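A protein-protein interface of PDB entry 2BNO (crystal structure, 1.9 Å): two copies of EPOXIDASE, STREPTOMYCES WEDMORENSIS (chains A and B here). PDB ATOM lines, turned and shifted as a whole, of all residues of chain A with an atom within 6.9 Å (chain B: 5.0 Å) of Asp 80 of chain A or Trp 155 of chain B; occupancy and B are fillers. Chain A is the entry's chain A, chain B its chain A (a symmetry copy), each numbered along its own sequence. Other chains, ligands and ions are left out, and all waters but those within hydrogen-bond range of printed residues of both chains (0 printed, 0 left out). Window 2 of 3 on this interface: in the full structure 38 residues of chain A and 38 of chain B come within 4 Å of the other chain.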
ATOM      1  N   ASN A  76      12.470  19.226 -23.685  1.00  0.00           N
ATOM      2  CA  ASN A  76      13.597  19.116 -22.761  1.00  0.00           C
ATOM      3  C   ASN A  76      14.232  17.761 -22.956  1.00  0.00           C
ATOM      4  O   ASN A  76      13.575  16.759 -22.740  1.00  0.00           O
ATOM      5  CB  ASN A  76      13.099  19.247 -21.336  1.00  0.00           C
ATOM      6  CG  ASN A  76      14.226  19.521 -20.359  1.00  0.00           C
ATOM      7  OD1 ASN A  76      15.316  18.992 -20.507  1.00  0.00           O
ATOM      8  ND2 ASN A  76      13.971  20.370 -19.373  1.00  0.00           N
ATOM      9  N   LEU A  78      17.291  17.035 -21.536  1.00  0.00           N
ATOM     10  CA  LEU A  78      18.357  17.026 -20.543  1.00  0.00           C
ATOM     11  C   LEU A  78      18.099  16.005 -19.438  1.00  0.00           C
ATOM     12  O   LEU A  78      16.951  15.755 -19.089  1.00  0.00           O
ATOM     13  CB  LEU A  78      18.448  18.414 -19.917  1.00  0.00           C
ATOM     14  CG  LEU A  78      18.708  19.568 -20.897  1.00  0.00           C
ATOM     15  CD1 LEU A  78      18.952  20.828 -20.121  1.00  0.00           C
ATOM     16  CD2 LEU A  78      19.904  19.275 -21.807  1.00  0.00           C
ATOM     17  N   ASP A  79      19.170  15.470 -18.868  1.00  0.00           N
ATOM     18  CA  ASP A  79      19.129  14.566 -17.729  1.00  0.00           C
ATOM     19  C   ASP A  79      19.501  15.371 -16.492  1.00  0.00           C
ATOM     20  O   ASP A  79      20.696  15.630 -16.238  1.00  0.00           O
ATOM     21  CB  ASP A  79      20.121  13.422 -17.954  1.00  0.00           C
ATOM     22  CG  ASP A  79      20.196  12.421 -16.750  1.00  0.00           C
ATOM     23  OD1 ASP A  79      19.342  12.507 -15.838  1.00  0.00           O
ATOM     24  OD2 ASP A  79      21.107  11.549 -16.647  1.00  0.00           O
ATOM     25  N   ASP A  80      18.492  15.809 -15.739  1.00  0.00           N
ATOM     26  CA  ASP A  80      18.719  16.763 -14.633  1.00  0.00           C
ATOM     27  C   ASP A  80      19.630  17.948 -15.001  1.00  0.00           C
ATOM     28  O   ASP A  80      20.554  18.307 -14.226  1.00  0.00           O
ATOM     29  CB  ASP A  80      19.314  16.025 -13.416  1.00  0.00           C
ATOM     30  CG  ASP A  80      18.309  15.118 -12.733  1.00  0.00           C
ATOM     31  OD1 ASP A  80      17.182  14.946 -13.253  1.00  0.00           O
ATOM     32  OD2 ASP A  80      18.572  14.539 -11.662  1.00  0.00           O
ATOM     33  N   GLY A  81      19.349  18.587 -16.146  1.00  0.00           N
ATOM     34  CA  GLY A  81      20.041  19.804 -16.533  1.00  0.00           C
ATOM     35  C   GLY A  81      21.272  19.625 -17.399  1.00  0.00           C
ATOM     36  O   GLY A  81      21.917  20.611 -17.772  1.00  0.00           O
ATOM     37  N   VAL A  82      21.587  18.378 -17.738  1.00  0.00           N
ATOM     38  CA  VAL A  82      22.845  18.057 -18.443  1.00  0.00           C
ATOM     39  C   VAL A  82      22.584  17.122 -19.605  1.00  0.00           C
ATOM     40  O   VAL A  82      21.687  16.284 -19.513  1.00  0.00           O
ATOM     41  CB  VAL A  82      23.878  17.437 -17.437  1.00  0.00           C
ATOM     42  CG1 VAL A  82      25.066  16.790 -18.151  1.00  0.00           C
ATOM     43  CG2 VAL A  82      24.394  18.529 -16.469  1.00  0.00           C
ATOM     44  N   ILE A  83      23.366  17.251 -20.683  1.00  0.00           N
ATOM     45  CA  ILE A  83      23.392  16.257 -21.747  1.00  0.00           C
ATOM     46  C   ILE A  83      24.852  16.060 -22.151  1.00  0.00           C
ATOM     47  O   ILE A  83      25.647  17.042 -22.233  1.00  0.00           O
ATOM     48  CB  ILE A  83      22.477  16.618 -22.960  1.00  0.00           C
ATOM     49  CG1 ILE A  83      22.605  15.597 -24.101  1.00  0.00           C
ATOM     50  CG2 ILE A  83      22.768  18.063 -23.520  1.00  0.00           C
ATOM     51  CD1 ILE A  83      21.319  15.533 -25.033  1.00  0.00           C
ATOM     52  N   ILE A  84      25.217  14.782 -22.307  1.00  0.00           N
ATOM     53  CA  ILE A  84      26.582  14.420 -22.699  1.00  0.00           C
ATOM     54  C   ILE A  84      26.596  13.726 -24.035  1.00  0.00           C
ATOM     55  O   ILE A  84      25.615  13.082 -24.425  1.00  0.00           O
ATOM     56  CB  ILE A  84      27.293  13.620 -21.589  1.00  0.00           C
ATOM     57  CG1 ILE A  84      26.683  12.210 -21.428  1.00  0.00           C
ATOM     58  CG2 ILE A  84      27.246  14.418 -20.270  1.00  0.00           C
ATOM     59  CD1 ILE A  84      27.706  11.066 -21.105  1.00  0.00           C
ATOM     60  N   PHE B 134      31.219  20.746  -5.239  1.00  0.00           N
ATOM     61  CA  PHE B 134      30.141  21.254  -6.068  1.00  0.00           C
ATOM     62  C   PHE B 134      30.065  22.758  -5.991  1.00  0.00           C
ATOM     63  O   PHE B 134      30.041  23.322  -4.893  1.00  0.00           O
ATOM     64  CB  PHE B 134      28.806  20.685  -5.591  1.00  0.00           C
ATOM     65  CG  PHE B 134      28.453  19.370  -6.215  1.00  0.00           C
ATOM     66  CD1 PHE B 134      29.191  18.228  -5.923  1.00  0.00           C
ATOM     67  CD2 PHE B 134      27.380  19.280  -7.102  1.00  0.00           C
ATOM     68  CE1 PHE B 134      28.854  17.003  -6.512  1.00  0.00           C
ATOM     69  CE2 PHE B 134      27.037  18.069  -7.690  1.00  0.00           C
ATOM     70  CZ  PHE B 134      27.777  16.927  -7.389  1.00  0.00           C
ATOM     71  N   MET B 153      32.655  13.581 -14.013  1.00  0.00           N
ATOM     72  CA  MET B 153      31.738  14.681 -13.808  1.00  0.00           C
ATOM     73  C   MET B 153      30.621  14.303 -12.815  1.00  0.00           C
ATOM     74  O   MET B 153      30.097  13.167 -12.845  1.00  0.00           O
ATOM     75  CB  MET B 153      31.152  15.132 -15.168  1.00  0.00           C
ATOM     76  CG  MET B 153      30.085  16.217 -15.087  1.00  0.00           C
ATOM     77  SD  MET B 153      30.756  17.816 -14.581  1.00  0.00           S
ATOM     78  CE  MET B 153      31.839  18.192 -15.963  1.00  0.00           C
ATOM     79  N   LYS B 154      30.285  15.217 -11.904  1.00  0.00           N
ATOM     80  CA  LYS B 154      29.085  15.057 -11.062  1.00  0.00           C
ATOM     81  C   LYS B 154      28.147  16.232 -11.220  1.00  0.00           C
ATOM     82  O   LYS B 154      28.601  17.366 -11.393  1.00  0.00           O
ATOM     83  CB  LYS B 154      29.440  14.872  -9.561  1.00  0.00           C
ATOM     84  CG  LYS B 154      30.487  13.757  -9.323  1.00  0.00           C
ATOM     85  CD  LYS B 154      30.760  13.548  -7.827  1.00  0.00           C
ATOM     86  CE  LYS B 154      31.623  12.304  -7.575  1.00  0.00           C
ATOM     87  NZ  LYS B 154      31.912  12.226  -6.113  1.00  0.00           N
ATOM     88  N   TRP B 155      26.838  15.986 -11.145  1.00  0.00           N
ATOM     89  CA  TRP B 155      25.898  17.095 -11.220  1.00  0.00           C
ATOM     90  C   TRP B 155      24.587  16.805 -10.509  1.00  0.00           C
ATOM     91  O   TRP B 155      24.288  15.655 -10.165  1.00  0.00           O
ATOM     92  CB  TRP B 155      25.642  17.507 -12.686  1.00  0.00           C
ATOM     93  CG  TRP B 155      24.774  16.557 -13.464  1.00  0.00           C
ATOM     94  CD1 TRP B 155      23.411  16.654 -13.650  1.00  0.00           C
ATOM     95  CD2 TRP B 155      25.206  15.478 -14.289  1.00  0.00           C
ATOM     96  NE1 TRP B 155      22.970  15.648 -14.480  1.00  0.00           N
ATOM     97  CE2 TRP B 155      24.046  14.911 -14.888  1.00  0.00           C
ATOM     98  CE3 TRP B 155      26.446  14.870 -14.535  1.00  0.00           C
ATOM     99  CZ2 TRP B 155      24.110  13.805 -15.720  1.00  0.00           C
ATOM    100  CZ3 TRP B 155      26.504  13.754 -15.364  1.00  0.00           C
ATOM    101  CH2 TRP B 155      25.347  13.238 -15.952  1.00  0.00           C
ATOM    102  N   GLY B 156      23.814  17.866 -10.300  1.00  0.00           N
ATOM    103  CA  GLY B 156      22.512  17.775  -9.656  1.00  0.00           C
ATOM    104  C   GLY B 156      22.643  17.977  -8.161  1.00  0.00           C
ATOM    105  O   GLY B 156      23.253  18.955  -7.701  1.00  0.00           O
ATOM    106  N   ASP B 157      22.082  17.033  -7.414  1.00  0.00           N
ATOM    107  CA  ASP B 157      22.129  17.021  -5.965  1.00  0.00           C
ATOM    108  C   ASP B 157      23.456  16.487  -5.453  1.00  0.00           C
ATOM    109  O   ASP B 157      23.758  15.303  -5.624  1.00  0.00           O
ATOM    110  CB  ASP B 157      21.013  16.102  -5.469  1.00  0.00           C
ATOM    111  CG  ASP B 157      20.867  16.107  -3.964  1.00  0.00           C
ATOM    112  OD1 ASP B 157      21.688  16.738  -3.260  1.00  0.00           O
ATOM    113  OD2 ASP B 157      19.956  15.468  -3.400  1.00  0.00           O
ATOM    114  N   PRO B 161      24.398  12.493  -6.543  1.00  0.00           N
ATOM    115  CA  PRO B 161      24.590  13.145  -7.823  1.00  0.00           C
ATOM    116  C   PRO B 161      24.412  12.204  -9.009  1.00  0.00           C
ATOM    117  O   PRO B 161      24.618  10.988  -8.898  1.00  0.00           O
ATOM    118  CB  PRO B 161      26.046  13.635  -7.744  1.00  0.00           C
ATOM    119  CG  PRO B 161      26.728  12.617  -6.875  1.00  0.00           C
ATOM    120  CD  PRO B 161      25.682  12.151  -5.897  1.00  0.00           C
ATOM    121  N   LYS B 162      24.096  12.793 -10.153  1.00  0.00           N
ATOM    122  CA  LYS B 162      24.245  12.140 -11.411  1.00  0.00           C
ATOM    123  C   LYS B 162      25.743  12.211 -11.729  1.00  0.00           C
ATOM    124  O   LYS B 162      26.431  13.128 -11.282  1.00  0.00           O
ATOM    125  CB  LYS B 162      23.460  12.917 -12.464  1.00  0.00           C
ATOM    126  CG  LYS B 162      21.941  13.010 -12.192  1.00  0.00           C
ATOM    127  CD  LYS B 162      21.260  11.677 -12.394  1.00  0.00           C
ATOM    128  CE  LYS B 162      19.738  11.822 -12.373  1.00  0.00           C
ATOM    129  NZ  LYS B 162      19.045  11.055 -13.463  1.00  0.00           N
ATOM    130  N   GLU B 163      26.245  11.254 -12.499  1.00  0.00           N
ATOM    131  CA  GLU B 163      27.680  11.130 -12.738  1.00  0.00           C
ATOM    132  C   GLU B 163      27.967  10.651 -14.148  1.00  0.00           C
ATOM    133  O   GLU B 163      27.137   9.979 -14.773  1.00  0.00           O
ATOM    134  CB  GLU B 163      28.299  10.133 -11.747  1.00  0.00           C
ATOM    135  CG  GLU B 163      28.085  10.446 -10.275  1.00  0.00           C
ATOM    136  CD  GLU B 163      28.835   9.466  -9.385  1.00  0.00           C
ATOM    137  OE1 GLU B 163      30.014   9.737  -9.102  1.00  0.00           O
ATOM    138  OE2 GLU B 163      28.245   8.427  -8.999  1.00  0.00           O
ATOM    139  N   ALA B 164      29.163  10.930 -14.635  1.00  0.00           N
ATOM    140  CA  ALA B 164      29.564  10.438 -15.937  1.00  0.00           C
ATOM    141  C   ALA B 164      31.066  10.441 -16.021  1.00  0.00           C
ATOM    142  O   ALA B 164      31.702  11.428 -15.615  1.00  0.00           O
ATOM    143  CB  ALA B 164      28.984  11.320 -17.068  1.00  0.00           C
ATOM    144  N   MET B 172      29.804  18.152 -23.407  1.00  0.00           N
ATOM    145  CA  MET B 172      28.747  18.228 -22.424  1.00  0.00           C
ATOM    146  C   MET B 172      28.101  19.602 -22.443  1.00  0.00           C
ATOM    147  O   MET B 172      28.753  20.605 -22.766  1.00  0.00           O
ATOM    148  CB  MET B 172      29.306  17.918 -21.052  1.00  0.00           C
ATOM    149  CG  MET B 172      28.313  18.014 -19.954  1.00  0.00           C
ATOM    150  SD  MET B 172      29.036  17.286 -18.485  1.00  0.00           S
ATOM    151  CE  MET B 172      28.329  18.309 -17.217  1.00  0.00           C
ATOM    152  N   VAL B 178      22.464  24.637 -12.703  1.00  0.00           N
ATOM    153  CA  VAL B 178      22.684  23.232 -12.328  1.00  0.00           C
ATOM    154  C   VAL B 178      24.009  23.079 -11.593  1.00  0.00           C
ATOM    155  O   VAL B 178      25.042  23.403 -12.163  1.00  0.00           O
ATOM    156  CB  VAL B 178      22.631  22.308 -13.590  1.00  0.00           C
ATOM    157  CG1 VAL B 178      23.027  20.836 -13.292  1.00  0.00           C
ATOM    158  CG2 VAL B 178      21.254  22.432 -14.309  1.00  0.00           C
ATOM    159  N   PRO B 179      24.011  22.601 -10.339  1.00  0.00           N
ATOM    160  CA  PRO B 179      25.268  22.403  -9.616  1.00  0.00           C
ATOM    161  C   PRO B 179      26.087  21.313 -10.287  1.00  0.00           C
ATOM    162  O   PRO B 179      25.521  20.325 -10.805  1.00  0.00           O
ATOM    163  CB  PRO B 179      24.806  21.921  -8.223  1.00  0.00           C
ATOM    164  CG  PRO B 179      23.380  22.390  -8.119  1.00  0.00           C
ATOM    165  CD  PRO B 179      22.838  22.266  -9.508  1.00  0.00           C
ATOM    166  N   HIS B 180      27.399  21.487 -10.321  1.00  0.00           N
ATOM    167  CA  HIS B 180      28.265  20.482 -10.924  1.00  0.00           C
ATOM    168  C   HIS B 180      29.678  20.597 -10.390  1.00  0.00           C
ATOM    169  O   HIS B 180      30.055  21.649  -9.882  1.00  0.00           O
ATOM    170  CB  HIS B 180      28.257  20.571 -12.463  1.00  0.00           C
ATOM    171  CG  HIS B 180      28.607  21.925 -12.983  1.00  0.00           C
ATOM    172  ND1 HIS B 180      27.747  23.002 -12.901  1.00  0.00           N
ATOM    173  CD2 HIS B 180      29.728  22.380 -13.587  1.00  0.00           C
ATOM    174  CE1 HIS B 180      28.333  24.068 -13.421  1.00  0.00           C
ATOM    175  NE2 HIS B 180      29.539  23.716 -13.835  1.00  0.00           N
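Among the printed residues, merely in contact across the chains: Ile 83 of chain A with Met 172 of chain B, Asp 80 of chain A with Trp 155 of chain B, Val 82 of chain A with Trp 155 of chain B, Gly 81 of chain A with Val 178 of chain B, Asp 80 of chain A with Val 178 of chain B, Val 82 of chain A with Met 172 of chain B and Ile 84 of chain A with Met 172 of chain B.
Of chain B, only Trp 155 (3.4 Å), Lys 162 (3.0 Å) and Val 178 (3.7 Å) come within 4 Å of Asp 80 of chain A. Trp 155 of chain B touches three residues of chain A. Printed residues of chain B within 4 Å of Gly 81 of chain A: Val 178. Printed residues of chain B within 4 Å of Ile 84 of chain A: Met 172. Printed residues of chain A within 4 Å of Met 172 of chain B: Val 82, Ile 83 and Ile 84. Asn 76 of chain A touches none of the printed residues of chain B. Pro 161 of chain B touches none of the printed residues of chain A. The nearest printed residue of chain B that does not touch Asp 80 of chain A is Gly 156 of chain B (5.0 Å). The nearest printed residue of chain A that does not touch Met 172 of chain B is Gly 81 of chain A (6.8 Å).
The backbone NH of Lys 162 of chain B lies within hydrogen-bond range of the backbone carbonyl oxygen of Trp 155 of chain B, at 2.9 Å. O of Val 178 of chain B sits at hydrogen-bond distance from ND1 of His 180 of chain B, 2.8 Å away.
No position is printed for both chains. Of the 10 pairs that touch across the chains among the printed residues, none has its exchanged pair printed and touching as well.
O of Asp 79 of chain A lies within hydrogen-bond range of NE1 of Trp 155 of chain B (2.9 Å). The side-chain carboxylate of Asp 79 of chain A lies within salt-bridge range of the side-chain amino group of Lys 162 of chain B, at 2.8 Å. OD2 of Asp 80 of chain A lies within salt-bridge range of NZ of Lys 162 of chain B, 3.95 Å away.
Hydrophobic or aromatic side chains of chain A that line the printed part of chain B: Val 82 and Ile 84. Along chain A the printed residues that touch a printed residue of chain B span positions 79 to 84. Of the 14 printed residues of chain B, 4 touch a printed residue of chain A. Printed residues of chain B that touch a printed residue of chain A: Trp 155, Lys 162, Met 172 and Val 178. Hydrophobic or aromatic side chains of chain B that line the printed part of chain A: Trp 155, Met 172 and Val 178. Among the printed residues, 10 pairs touch across the chains. Among the printed residues, Asp or Glu carboxylates within 4 Å of a Lys or Arg side-chain nitrogen of the other chain: Asp 79 of chain A with Lys 162 of chain B (2.8 Å) and Asp 80 of chain A with Lys 162 of chain B (3.95 Å).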
